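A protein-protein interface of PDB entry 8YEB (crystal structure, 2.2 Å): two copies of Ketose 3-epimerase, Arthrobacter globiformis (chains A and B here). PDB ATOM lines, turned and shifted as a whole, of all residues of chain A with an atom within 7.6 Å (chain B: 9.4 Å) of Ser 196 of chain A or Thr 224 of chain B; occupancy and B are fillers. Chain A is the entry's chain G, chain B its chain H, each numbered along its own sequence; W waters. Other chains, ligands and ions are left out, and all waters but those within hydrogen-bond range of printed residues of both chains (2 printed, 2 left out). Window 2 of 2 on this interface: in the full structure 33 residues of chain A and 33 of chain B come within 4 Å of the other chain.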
ATOM      1  N   THR A 166       3.607 -12.553   1.540  1.00  0.00           N
ATOM      2  CA  THR A 166       3.729 -13.711   0.666  1.00  0.00           C
ATOM      3  C   THR A 166       4.496 -13.365  -0.606  1.00  0.00           C
ATOM      4  O   THR A 166       4.541 -12.209  -1.049  1.00  0.00           O
ATOM      5  CB  THR A 166       2.359 -14.242   0.233  1.00  0.00           C
ATOM      6  OG1 THR A 166       1.807 -13.274  -0.660  1.00  0.00           O
ATOM      7  CG2 THR A 166       1.446 -14.500   1.414  1.00  0.00           C
ATOM      8  N   MET A 191       8.274 -18.252   5.188  1.00  0.00           N
ATOM      9  CA  MET A 191       7.432 -19.044   4.298  1.00  0.00           C
ATOM     10  C   MET A 191       6.625 -20.045   5.113  1.00  0.00           C
ATOM     11  O   MET A 191       5.464 -20.292   4.830  1.00  0.00           O
ATOM     12  CB  MET A 191       8.285 -19.827   3.292  1.00  0.00           C
ATOM     13  CG  MET A 191       8.911 -18.937   2.249  1.00  0.00           C
ATOM     14  SD  MET A 191      10.107 -19.827   1.242  1.00  0.00           S
ATOM     15  CE  MET A 191       9.023 -20.766   0.183  1.00  0.00           C
ATOM     16  N   ASN A 192       7.267 -20.590   6.143  1.00  0.00           N
ATOM     17  CA  ASN A 192       6.693 -21.629   6.980  1.00  0.00           C
ATOM     18  C   ASN A 192       5.386 -21.172   7.640  1.00  0.00           C
ATOM     19  O   ASN A 192       4.549 -22.016   7.988  1.00  0.00           O
ATOM     20  CB  ASN A 192       7.724 -22.037   8.030  1.00  0.00           C
ATOM     21  CG  ASN A 192       7.340 -23.271   8.806  1.00  0.00           C
ATOM     22  OD1 ASN A 192       7.048 -24.320   8.223  1.00  0.00           O
ATOM     23  ND2 ASN A 192       7.330 -23.127  10.117  1.00  0.00           N
ATOM     24  N   ILE A 193       5.212 -19.849   7.797  1.00  0.00           N
ATOM     25  CA  ILE A 193       4.013 -19.274   8.385  1.00  0.00           C
ATOM     26  C   ILE A 193       3.010 -18.920   7.291  1.00  0.00           C
ATOM     27  O   ILE A 193       1.909 -19.443   7.307  1.00  0.00           O
ATOM     28  CB  ILE A 193       4.371 -18.076   9.295  1.00  0.00           C
ATOM     29  CG1 ILE A 193       5.272 -18.545  10.450  1.00  0.00           C
ATOM     30  CG2 ILE A 193       3.100 -17.377   9.780  1.00  0.00           C
ATOM     31  CD1 ILE A 193       6.088 -17.452  11.110  1.00  0.00           C
ATOM     32  N   GLU A 194       3.414 -18.123   6.308  1.00  0.00           N
ATOM     33  CA  GLU A 194       2.465 -17.415   5.466  1.00  0.00           C
ATOM     34  C   GLU A 194       2.062 -18.187   4.207  1.00  0.00           C
ATOM     35  O   GLU A 194       0.908 -18.042   3.760  1.00  0.00           O
ATOM     36  CB  GLU A 194       3.012 -16.031   5.104  1.00  0.00           C
ATOM     37  CG  GLU A 194       3.305 -15.145   6.321  1.00  0.00           C
ATOM     38  CD  GLU A 194       2.088 -14.710   7.125  1.00  0.00           C
ATOM     39  OE1 GLU A 194       0.965 -14.893   6.620  1.00  0.00           O
ATOM     40  OE2 GLU A 194       2.271 -14.231   8.296  1.00  0.00           O
ATOM     41  N   GLU A 195       2.966 -19.019   3.664  1.00  0.00           N
ATOM     42  CA  GLU A 195       2.749 -19.606   2.350  1.00  0.00           C
ATOM     43  C   GLU A 195       1.916 -20.888   2.421  1.00  0.00           C
ATOM     44  O   GLU A 195       1.816 -21.530   3.457  1.00  0.00           O
ATOM     45  CB  GLU A 195       4.087 -19.931   1.682  1.00  0.00           C
ATOM     46  CG  GLU A 195       4.983 -18.721   1.485  1.00  0.00           C
ATOM     47  CD  GLU A 195       4.575 -17.653   0.478  1.00  0.00           C
ATOM     48  OE1 GLU A 195       3.565 -17.810  -0.221  1.00  0.00           O
ATOM     49  OE2 GLU A 195       5.312 -16.654   0.384  1.00  0.00           O
ATOM     50  N   SER A 196       1.362 -21.278   1.273  1.00  0.00           N
ATOM     51  CA  SER A 196       0.536 -22.472   1.165  1.00  0.00           C
ATOM     52  C   SER A 196       1.386 -23.739   1.259  1.00  0.00           C
ATOM     53  O   SER A 196       0.883 -24.792   1.650  1.00  0.00           O
ATOM     54  CB  SER A 196      -0.270 -22.448  -0.114  1.00  0.00           C
ATOM     55  OG  SER A 196       0.575 -22.416  -1.270  1.00  0.00           O
ATOM     56  N   ASP A 197       2.658 -23.640   0.864  1.00  0.00           N
ATOM     57  CA  ASP A 197       3.585 -24.758   0.823  1.00  0.00           C
ATOM     58  C   ASP A 197       4.966 -24.213   0.434  1.00  0.00           C
ATOM     59  O   ASP A 197       5.083 -23.013   0.203  1.00  0.00           O
ATOM     60  CB  ASP A 197       3.124 -25.796  -0.199  1.00  0.00           C
ATOM     61  CG  ASP A 197       3.010 -25.191  -1.586  1.00  0.00           C
ATOM     62  OD1 ASP A 197       4.073 -24.896  -2.193  1.00  0.00           O
ATOM     63  OD2 ASP A 197       1.873 -24.958  -2.015  1.00  0.00           O
ATOM     64  N   MET A 198       5.988 -25.076   0.318  1.00  0.00           N
ATOM     65  CA  MET A 198       7.338 -24.593   0.102  1.00  0.00           C
ATOM     66  C   MET A 198       7.777 -24.679  -1.363  1.00  0.00           C
ATOM     67  O   MET A 198       8.900 -24.307  -1.659  1.00  0.00           O
ATOM     68  CB  MET A 198       8.338 -25.369   0.962  1.00  0.00           C
ATOM     69  CG  MET A 198       8.058 -25.292   2.451  1.00  0.00           C
ATOM     70  SD  MET A 198       8.272 -23.618   3.149  1.00  0.00           S
ATOM     71  CE  MET A 198      10.038 -23.467   2.992  1.00  0.00           C
ATOM     72  N   PHE A 199       6.917 -25.086  -2.294  1.00  0.00           N
ATOM     73  CA  PHE A 199       7.305 -25.127  -3.700  1.00  0.00           C
ATOM     74  C   PHE A 199       6.621 -24.032  -4.536  1.00  0.00           C
ATOM     75  O   PHE A 199       7.285 -23.380  -5.345  1.00  0.00           O
ATOM     76  CB  PHE A 199       7.102 -26.531  -4.276  1.00  0.00           C
ATOM     77  CG  PHE A 199       5.678 -26.985  -4.533  1.00  0.00           C
ATOM     78  CD1 PHE A 199       4.940 -27.604  -3.541  1.00  0.00           C
ATOM     79  CD2 PHE A 199       5.095 -26.809  -5.777  1.00  0.00           C
ATOM     80  CE1 PHE A 199       3.643 -28.032  -3.780  1.00  0.00           C
ATOM     81  CE2 PHE A 199       3.787 -27.215  -6.019  1.00  0.00           C
ATOM     82  CZ  PHE A 199       3.075 -27.850  -5.023  1.00  0.00           C
ATOM     83  N   SER A 200       5.313 -23.801  -4.340  1.00  0.00           N
ATOM     84  CA  SER A 200       4.548 -22.835  -5.111  1.00  0.00           C
ATOM     85  C   SER A 200       5.240 -21.480  -5.147  1.00  0.00           C
ATOM     86  O   SER A 200       5.287 -20.824  -6.194  1.00  0.00           O
ATOM     87  CB  SER A 200       3.150 -22.640  -4.528  1.00  0.00           C
ATOM     88  OG  SER A 200       2.444 -23.840  -4.586  1.00  0.00           O
ATOM     89  N   PRO A 201       5.634 -20.928  -3.980  1.00  0.00           N
ATOM     90  CA  PRO A 201       6.242 -19.596  -3.958  1.00  0.00           C
ATOM     91  C   PRO A 201       7.513 -19.538  -4.820  1.00  0.00           C
ATOM     92  O   PRO A 201       7.775 -18.525  -5.482  1.00  0.00           O
ATOM     93  CB  PRO A 201       6.527 -19.374  -2.472  1.00  0.00           C
ATOM     94  CG  PRO A 201       5.560 -20.294  -1.760  1.00  0.00           C
ATOM     95  CD  PRO A 201       5.540 -21.532  -2.642  1.00  0.00           C
ATOM     96  N   ASP A 204       6.328 -19.691  -8.554  1.00  0.00           N
ATOM     97  CA  ASP A 204       5.651 -18.457  -8.949  1.00  0.00           C
ATOM     98  C   ASP A 204       6.642 -17.307  -9.088  1.00  0.00           C
ATOM     99  O   ASP A 204       6.468 -16.444  -9.937  1.00  0.00           O
ATOM    100  CB  ASP A 204       4.567 -18.021  -7.958  1.00  0.00           C
ATOM    101  CG  ASP A 204       3.320 -18.881  -7.964  1.00  0.00           C
ATOM    102  OD1 ASP A 204       3.136 -19.645  -8.953  1.00  0.00           O
ATOM    103  OD2 ASP A 204       2.563 -18.817  -6.949  1.00  0.00           O
ATOM    104  N   GLY B 215      -5.293 -24.842  13.930  1.00  0.00           N
ATOM    105  CA  GLY B 215      -5.038 -23.674  13.116  1.00  0.00           C
ATOM    106  C   GLY B 215      -3.949 -23.979  12.093  1.00  0.00           C
ATOM    107  O   GLY B 215      -2.896 -24.514  12.432  1.00  0.00           O
ATOM    108  N   GLU B 216      -4.240 -23.634  10.841  1.00  0.00           N
ATOM    109  CA  GLU B 216      -3.266 -23.739   9.769  1.00  0.00           C
ATOM    110  C   GLU B 216      -2.165 -22.691   9.952  1.00  0.00           C
ATOM    111  O   GLU B 216      -2.282 -21.720  10.730  1.00  0.00           O
ATOM    112  CB  GLU B 216      -3.953 -23.584   8.416  1.00  0.00           C
ATOM    113  CG  GLU B 216      -3.087 -23.932   7.222  1.00  0.00           C
ATOM    114  CD  GLU B 216      -2.423 -25.294   7.319  1.00  0.00           C
ATOM    115  OE1 GLU B 216      -1.300 -25.350   7.873  1.00  0.00           O
ATOM    116  OE2 GLU B 216      -3.026 -26.281   6.828  1.00  0.00           O
ATOM    117  N   SER B 217      -1.064 -22.923   9.238  1.00  0.00           N
ATOM    118  CA  SER B 217       0.147 -22.153   9.455  1.00  0.00           C
ATOM    119  C   SER B 217      -0.109 -20.654   9.270  1.00  0.00           C
ATOM    120  O   SER B 217       0.507 -19.839   9.944  1.00  0.00           O
ATOM    121  CB  SER B 217       1.240 -22.650   8.563  1.00  0.00           C
ATOM    122  OG  SER B 217       0.865 -22.500   7.218  1.00  0.00           O
ATOM    123  N   HIS B 218      -1.001 -20.313   8.340  1.00  0.00           N
ATOM    124  CA  HIS B 218      -1.359 -18.944   8.046  1.00  0.00           C
ATOM    125  C   HIS B 218      -2.771 -18.596   8.548  1.00  0.00           C
ATOM    126  O   HIS B 218      -3.265 -17.526   8.229  1.00  0.00           O
ATOM    127  CB  HIS B 218      -1.249 -18.733   6.536  1.00  0.00           C
ATOM    128  CG  HIS B 218      -2.064 -19.710   5.765  1.00  0.00           C
ATOM    129  ND1 HIS B 218      -3.255 -20.237   6.221  1.00  0.00           N
ATOM    130  CD2 HIS B 218      -1.849 -20.245   4.561  1.00  0.00           C
ATOM    131  CE1 HIS B 218      -3.724 -21.065   5.311  1.00  0.00           C
ATOM    132  NE2 HIS B 218      -2.862 -21.107   4.311  1.00  0.00           N
ATOM    133  N   ARG B 219      -3.407 -19.511   9.299  1.00  0.00           N
ATOM    134  CA  ARG B 219      -4.673 -19.316  10.011  1.00  0.00           C
ATOM    135  C   ARG B 219      -5.857 -19.287   9.038  1.00  0.00           C
ATOM    136  O   ARG B 219      -6.940 -18.850   9.408  1.00  0.00           O
ATOM    137  CB  ARG B 219      -4.664 -18.068  10.913  1.00  0.00           C
ATOM    138  CG  ARG B 219      -3.481 -18.021  11.866  1.00  0.00           C
ATOM    139  CD  ARG B 219      -3.503 -17.057  13.034  1.00  0.00           C
ATOM    140  NE  ARG B 219      -3.992 -17.720  14.231  1.00  0.00           N
ATOM    141  CZ  ARG B 219      -3.807 -17.308  15.478  1.00  0.00           C
ATOM    142  NH1 ARG B 219      -4.170 -18.103  16.461  1.00  0.00           N
ATOM    143  NH2 ARG B 219      -3.218 -16.152  15.754  1.00  0.00           N
ATOM    144  N   GLY B 220      -5.693 -19.859   7.841  1.00  0.00           N
ATOM    145  CA  GLY B 220      -6.798 -19.990   6.895  1.00  0.00           C
ATOM    146  C   GLY B 220      -7.401 -21.398   6.870  1.00  0.00           C
ATOM    147  O   GLY B 220      -7.497 -22.063   7.905  1.00  0.00           O
ATOM    148  N   TYR B 221      -7.785 -21.864   5.670  1.00  0.00           N
ATOM    149  CA  TYR B 221      -8.367 -23.186   5.490  1.00  0.00           C
ATOM    150  C   TYR B 221      -7.403 -24.265   5.972  1.00  0.00           C
ATOM    151  O   TYR B 221      -6.205 -24.191   5.727  1.00  0.00           O
ATOM    152  CB  TYR B 221      -8.691 -23.450   4.017  1.00  0.00           C
ATOM    153  CG  TYR B 221     -10.074 -23.053   3.544  1.00  0.00           C
ATOM    154  CD1 TYR B 221     -10.385 -21.744   3.204  1.00  0.00           C
ATOM    155  CD2 TYR B 221     -11.081 -23.999   3.401  1.00  0.00           C
ATOM    156  CE1 TYR B 221     -11.657 -21.379   2.780  1.00  0.00           C
ATOM    157  CE2 TYR B 221     -12.356 -23.653   2.969  1.00  0.00           C
ATOM    158  CZ  TYR B 221     -12.642 -22.342   2.634  1.00  0.00           C
ATOM    159  OH  TYR B 221     -13.912 -21.996   2.202  1.00  0.00           O
ATOM    160  N   LEU B 222      -7.933 -25.284   6.655  1.00  0.00           N
ATOM    161  CA  LEU B 222      -7.121 -26.401   7.112  1.00  0.00           C
ATOM    162  C   LEU B 222      -6.623 -27.221   5.923  1.00  0.00           C
ATOM    163  O   LEU B 222      -7.402 -27.587   5.057  1.00  0.00           O
ATOM    164  CB  LEU B 222      -7.972 -27.245   8.062  1.00  0.00           C
ATOM    165  CG  LEU B 222      -8.459 -26.505   9.315  1.00  0.00           C
ATOM    166  CD1 LEU B 222      -9.116 -27.459  10.282  1.00  0.00           C
ATOM    167  CD2 LEU B 222      -7.313 -25.769  10.009  1.00  0.00           C
ATOM    168  N   GLY B 223      -5.315 -27.503   5.890  1.00  0.00           N
ATOM    169  CA  GLY B 223      -4.725 -28.314   4.832  1.00  0.00           C
ATOM    170  C   GLY B 223      -4.237 -27.484   3.644  1.00  0.00           C
ATOM    171  O   GLY B 223      -3.994 -28.029   2.551  1.00  0.00           O
ATOM    172  N   THR B 224      -4.114 -26.160   3.850  1.00  0.00           N
ATOM    173  CA  THR B 224      -3.677 -25.267   2.781  1.00  0.00           C
ATOM    174  C   THR B 224      -2.391 -24.524   3.159  1.00  0.00           C
ATOM    175  O   THR B 224      -2.078 -23.481   2.593  1.00  0.00           O
ATOM    176  CB  THR B 224      -4.793 -24.283   2.425  1.00  0.00           C
ATOM    177  OG1 THR B 224      -4.964 -23.416   3.551  1.00  0.00           O
ATOM    178  CG2 THR B 224      -6.081 -24.996   2.067  1.00  0.00           C
ATOM    179  N   GLY B 225      -1.667 -25.056   4.139  1.00  0.00           N
ATOM    180  CA  GLY B 225      -0.468 -24.421   4.656  1.00  0.00           C
ATOM    181  C   GLY B 225       0.506 -25.512   5.061  1.00  0.00           C
ATOM    182  O   GLY B 225       0.397 -26.632   4.562  1.00  0.00           O
ATOM    183  N   SER B 226       1.411 -25.200   5.983  1.00  0.00           N
ATOM    184  CA  SER B 226       2.544 -26.071   6.244  1.00  0.00           C
ATOM    185  C   SER B 226       2.405 -26.828   7.573  1.00  0.00           C
ATOM    186  O   SER B 226       3.342 -27.521   7.981  1.00  0.00           O
ATOM    187  CB  SER B 226       3.797 -25.243   6.215  1.00  0.00           C
ATOM    188  OG  SER B 226       3.874 -24.468   7.395  1.00  0.00           O
ATOM    189  N   VAL B 227       1.256 -26.704   8.277  1.00  0.00           N
ATOM    190  CA  VAL B 227       1.111 -27.412   9.545  1.00  0.00           C
ATOM    191  C   VAL B 227       1.041 -28.924   9.311  1.00  0.00           C
ATOM    192  O   VAL B 227       0.302 -29.390   8.459  1.00  0.00           O
ATOM    193  CB  VAL B 227      -0.086 -26.907  10.376  1.00  0.00           C
ATOM    194  CG1 VAL B 227      -0.469 -27.879  11.496  1.00  0.00           C
ATOM    195  CG2 VAL B 227       0.224 -25.543  10.981  1.00  0.00           C
ATOM    196  N   ASP B 228       1.819 -29.678  10.096  1.00  0.00           N
ATOM    197  CA  ASP B 228       1.847 -31.130  10.026  1.00  0.00           C
ATOM    198  C   ASP B 228       0.734 -31.657  10.940  1.00  0.00           C
ATOM    199  O   ASP B 228       0.973 -32.136  12.055  1.00  0.00           O
ATOM    200  CB  ASP B 228       3.242 -31.695  10.359  1.00  0.00           C
ATOM    201  CG  ASP B 228       3.359 -33.221  10.378  1.00  0.00           C
ATOM    202  OD1 ASP B 228       2.389 -33.896   9.948  1.00  0.00           O
ATOM    203  OD2 ASP B 228       4.431 -33.745  10.819  1.00  0.00           O
ATOM    204  N   PHE B 229      -0.499 -31.578  10.436  1.00  0.00           N
ATOM    205  CA  PHE B 229      -1.651 -32.078  11.168  1.00  0.00           C
ATOM    206  C   PHE B 229      -1.579 -33.578  11.399  1.00  0.00           C
ATOM    207  O   PHE B 229      -2.030 -34.013  12.441  1.00  0.00           O
ATOM    208  CB  PHE B 229      -2.954 -31.716  10.458  1.00  0.00           C
ATOM    209  CG  PHE B 229      -3.308 -30.270  10.662  1.00  0.00           C
ATOM    210  CD1 PHE B 229      -3.537 -29.781  11.929  1.00  0.00           C
ATOM    211  CD2 PHE B 229      -3.410 -29.414   9.583  1.00  0.00           C
ATOM    212  CE1 PHE B 229      -3.822 -28.431  12.120  1.00  0.00           C
ATOM    213  CE2 PHE B 229      -3.706 -28.078   9.767  1.00  0.00           C
ATOM    214  CZ  PHE B 229      -3.918 -27.591  11.041  1.00  0.00           C
ATOM    215  N   PHE B 247     -11.449 -25.344  16.268  1.00  0.00           N
ATOM    216  CA  PHE B 247     -10.978 -24.683  15.065  1.00  0.00           C
ATOM    217  C   PHE B 247     -10.849 -23.187  15.304  1.00  0.00           C
ATOM    218  O   PHE B 247     -11.738 -22.572  15.892  1.00  0.00           O
ATOM    219  CB  PHE B 247     -11.949 -24.938  13.913  1.00  0.00           C
ATOM    220  CG  PHE B 247     -11.679 -24.176  12.645  1.00  0.00           C
ATOM    221  CD1 PHE B 247     -10.449 -24.260  12.013  1.00  0.00           C
ATOM    222  CD2 PHE B 247     -12.672 -23.425  12.049  1.00  0.00           C
ATOM    223  CE1 PHE B 247     -10.214 -23.593  10.824  1.00  0.00           C
ATOM    224  CE2 PHE B 247     -12.436 -22.764  10.854  1.00  0.00           C
ATOM    225  CZ  PHE B 247     -11.214 -22.855  10.242  1.00  0.00           C
ATOM    226  N   SER B 249      -9.650 -19.618  13.111  1.00  0.00           N
ATOM    227  CA  SER B 249      -9.288 -19.054  11.832  1.00  0.00           C
ATOM    228  C   SER B 249      -9.668 -17.570  11.756  1.00  0.00           C
ATOM    229  O   SER B 249     -10.690 -17.124  12.288  1.00  0.00           O
ATOM    230  CB  SER B 249      -9.913 -19.872  10.727  1.00  0.00           C
ATOM    231  OG  SER B 249      -9.589 -19.334   9.467  1.00  0.00           O
ATOM    232  N   ARG B 267      -4.448 -10.062   5.744  1.00  0.00           N
ATOM    233  CA  ARG B 267      -4.791 -10.667   4.455  1.00  0.00           C
ATOM    234  C   ARG B 267      -6.136 -11.377   4.545  1.00  0.00           C
ATOM    235  O   ARG B 267      -6.502 -11.879   5.596  1.00  0.00           O
ATOM    236  CB  ARG B 267      -3.799 -11.743   3.984  1.00  0.00           C
ATOM    237  CG  ARG B 267      -2.365 -11.287   3.768  1.00  0.00           C
ATOM    238  CD  ARG B 267      -1.385 -12.413   4.099  1.00  0.00           C
ATOM    239  NE  ARG B 267      -1.508 -13.500   3.157  1.00  0.00           N
ATOM    240  CZ  ARG B 267      -1.254 -14.789   3.384  1.00  0.00           C
ATOM    241  NH1 ARG B 267      -0.653 -15.218   4.479  1.00  0.00           N
ATOM    242  NH2 ARG B 267      -1.575 -15.661   2.447  1.00  0.00           N
ATOM    243  N   LEU B 269      -7.986 -14.608   3.853  1.00  0.00           N
ATOM    244  CA  LEU B 269      -7.723 -16.030   3.641  1.00  0.00           C
ATOM    245  C   LEU B 269      -9.002 -16.803   3.282  1.00  0.00           C
ATOM    246  O   LEU B 269      -8.938 -18.011   3.065  1.00  0.00           O
ATOM    247  CB  LEU B 269      -7.075 -16.621   4.905  1.00  0.00           C
ATOM    248  CG  LEU B 269      -5.541 -16.619   4.975  1.00  0.00           C
ATOM    249  CD1 LEU B 269      -4.910 -17.431   3.849  1.00  0.00           C
ATOM    250  CD2 LEU B 269      -5.026 -15.201   4.933  1.00  0.00           C
ATOM    251  N   TRP B 270     -10.161 -16.119   3.281  1.00  0.00           N
ATOM    252  CA  TRP B 270     -11.463 -16.700   2.977  1.00  0.00           C
ATOM    253  C   TRP B 270     -12.530 -15.612   3.039  1.00  0.00           C
ATOM    254  O   TRP B 270     -12.404 -14.674   3.825  1.00  0.00           O
ATOM    255  CB  TRP B 270     -11.822 -17.847   3.934  1.00  0.00           C
ATOM    256  CG  TRP B 270     -11.628 -17.569   5.400  1.00  0.00           C
ATOM    257  CD1 TRP B 270     -10.591 -17.993   6.185  1.00  0.00           C
ATOM    258  CD2 TRP B 270     -12.526 -16.880   6.291  1.00  0.00           C
ATOM    259  NE1 TRP B 270     -10.771 -17.604   7.487  1.00  0.00           N
ATOM    260  CE2 TRP B 270     -11.944 -16.912   7.586  1.00  0.00           C
ATOM    261  CE3 TRP B 270     -13.746 -16.216   6.127  1.00  0.00           C
ATOM    262  CZ2 TRP B 270     -12.551 -16.324   8.697  1.00  0.00           C
ATOM    263  CZ3 TRP B 270     -14.357 -15.654   7.233  1.00  0.00           C
ATOM    264  CH2 TRP B 270     -13.766 -15.705   8.499  1.00  0.00           C
ATOM    265  N   LEU B 276     -15.977 -22.550   5.077  1.00  0.00           N
ATOM    266  CA  LEU B 276     -14.750 -22.720   5.856  1.00  0.00           C
ATOM    267  C   LEU B 276     -15.046 -23.569   7.082  1.00  0.00           C
ATOM    268  O   LEU B 276     -14.337 -24.547   7.363  1.00  0.00           O
ATOM    269  CB  LEU B 276     -14.151 -21.359   6.261  1.00  0.00           C
ATOM    270  CG  LEU B 276     -12.995 -21.429   7.262  1.00  0.00           C
ATOM    271  CD1 LEU B 276     -11.694 -21.758   6.558  1.00  0.00           C
ATOM    272  CD2 LEU B 276     -12.833 -20.136   8.044  1.00  0.00           C
ATOM    273  N   HIS B 279     -15.953 -27.154   6.369  1.00  0.00           N
ATOM    274  CA  HIS B 279     -14.748 -27.854   5.938  1.00  0.00           C
ATOM    275  C   HIS B 279     -13.902 -28.217   7.152  1.00  0.00           C
ATOM    276  O   HIS B 279     -13.421 -29.339   7.257  1.00  0.00           O
ATOM    277  CB  HIS B 279     -13.992 -27.058   4.870  1.00  0.00           C
ATOM    278  CG  HIS B 279     -12.682 -27.680   4.520  1.00  0.00           C
ATOM    279  ND1 HIS B 279     -11.543 -27.541   5.284  1.00  0.00           N
ATOM    280  CD2 HIS B 279     -12.351 -28.460   3.473  1.00  0.00           C
ATOM    281  CE1 HIS B 279     -10.561 -28.231   4.702  1.00  0.00           C
ATOM    282  NE2 HIS B 279     -11.032 -28.799   3.601  1.00  0.00           N
ATOM    283  N   PHE B 283     -12.845 -31.691   8.654  1.00  0.00           N
ATOM    284  CA  PHE B 283     -11.407 -31.968   8.685  1.00  0.00           C
ATOM    285  C   PHE B 283     -11.028 -32.636  10.004  1.00  0.00           C
ATOM    286  O   PHE B 283     -10.359 -33.671  10.025  1.00  0.00           O
ATOM    287  CB  PHE B 283     -10.573 -30.691   8.479  1.00  0.00           C
ATOM    288  CG  PHE B 283      -9.073 -30.880   8.373  1.00  0.00           C
ATOM    289  CD1 PHE B 283      -8.282 -30.907   9.501  1.00  0.00           C
ATOM    290  CD2 PHE B 283      -8.448 -31.037   7.141  1.00  0.00           C
ATOM    291  CE1 PHE B 283      -6.904 -31.079   9.397  1.00  0.00           C
ATOM    292  CE2 PHE B 283      -7.067 -31.186   7.039  1.00  0.00           C
ATOM    293  CZ  PHE B 283      -6.292 -31.206   8.165  1.00  0.00           C
HETATM  294  O   HOH W   1       6.009 -26.581   9.102  1.00  0.00           O
HETATM  295  O   HOH W   2      -1.158 -18.055   2.227  1.00  0.00           O
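The side-chain hydroxyl of Ser 226 of chain B is in hydrogen-bond range of the backbone carbonyl oxygen of Asn 192 of chain A (2.6 Å). OG of Ser 217 of chain B lies close to O of Ile 193 of chain A (3.2 Å). The backbone NH of His 218 of chain B lies within hydrogen-bond range of the backbone carbonyl oxygen of Ile 193 of chain A (3.2 Å). The side-chain carboxylate (OE1) of Glu 194 of chain A lies within salt-bridge range of the guanidinium group (NH1) of Arg 267 of chain B (2.7 Å). The backbone carbonyl oxygen of Ser 196 of chain A lies close to the backbone carbonyl oxygen of Thr 224 of chain B. O of Gly 225 of chain B lies close to O of Ser 196 of chain A, at 3.5 Å.
The side-chain hydroxyl (OG) of Ser 196 of chain A is in hydrogen-bond range of the side-chain carboxylate (OD2) of Asp 197 of chain A (2.9 Å). OE2 of Glu 216 of chain B lies within hydrogen-bond range of N of Thr 224 of chain B, at 3.2 Å. N of Gly 225 of chain B lies within hydrogen-bond range of OE2 of Glu 216 of chain B, 3.3 Å away. The backbone NH (N) of Ser 226 of chain B sits at hydrogen-bond distance from the side-chain carboxylate (OE1) of Glu 216 of chain B (3.3 Å). A ring nitrogen (ND1) of His 218 of chain B lies within hydrogen-bond range of the backbone NH of Gly 220 of chain B (3.0 Å). The backbone carbonyl oxygen of Tyr 221 of chain B lies within hydrogen-bond range of the side-chain hydroxyl of Thr 224 of chain B (2.6 Å).
Among the printed residues, pairs that only touch across the chains: Thr 166 of chain A with Arg 267 of chain B, Asn 192 of chain A with Ser 217 of chain B, Glu 194 of chain A with His 218 of chain B, Glu 195 of chain A with Gly 225 of chain B and Glu 195 of chain A with Ser 217 of chain B.
Of the printed residues of chain B, Thr 166 of chain A touches Arg 267 (3.4 Å). Of the printed residues of chain B, Glu 195 of chain A touches Ser 217 and Gly 225. Of the printed residues of chain B, Ser 196 of chain A touches Thr 224 and Gly 225. No residue of chain B comes within 4 Å of Asp 197 of chain A. Phe 199 of chain A touches none of the printed residues of chain B. Printed residues of chain A within 4 Å of His 218 of chain B: Ile 193 (3.2 Å) and Glu 194 (3.6 Å). No residue of chain A comes within 4 Å of Gly 223 of chain B. Thr 224 of chain B touches just one residue of chain A: Ser 196 (3.1 Å). Gly 225 of chain B touches just these residues of chain A: Glu 195 (3.9 Å) and Ser 196 (3.3 Å). The nearest residue of chain A that does not touch Thr 224 of chain B is Glu 195 of chain A (4.4 Å). The nearest printed residue of chain A that does not touch Arg 267 of chain B is Glu 195 of chain A (5.3 Å).
Of the 23 printed residues of chain B, 6 touch a printed residue of chain A. Along chain B the printed residues that touch a printed residue of chain A span positions 217 to 267. Of the 13 printed residues of chain A, 6 touch a printed residue of chain B. Printed residues of chain A that touch a printed residue of chain B: Thr 166, Asn 192, Ile 193, Glu 194, Glu 195 and Ser 196. Hydrophobic or aromatic side chains of chain A that line the printed part of chain B: Ile 193. Among the printed residues, Asp or Glu carboxylates within 4 Å of a Lys or Arg side-chain nitrogen of the other chain: Glu 194 of chain A with Arg 267 of chain B.
No position is printed for both chains.
Water W2 lies within hydrogen-bond range of the guanidinium group (NH2) of Arg 267 of chain B (2.4 Å) and the backbone carbonyl oxygen (O) of Glu 194 of chain A (2.6 Å). Water W1 lies within hydrogen-bond range of the side-chain amide oxygen of Asn 192 of chain A (2.6 Å) and the backbone carbonyl oxygen of Ser 226 of chain B (3.0 Å).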
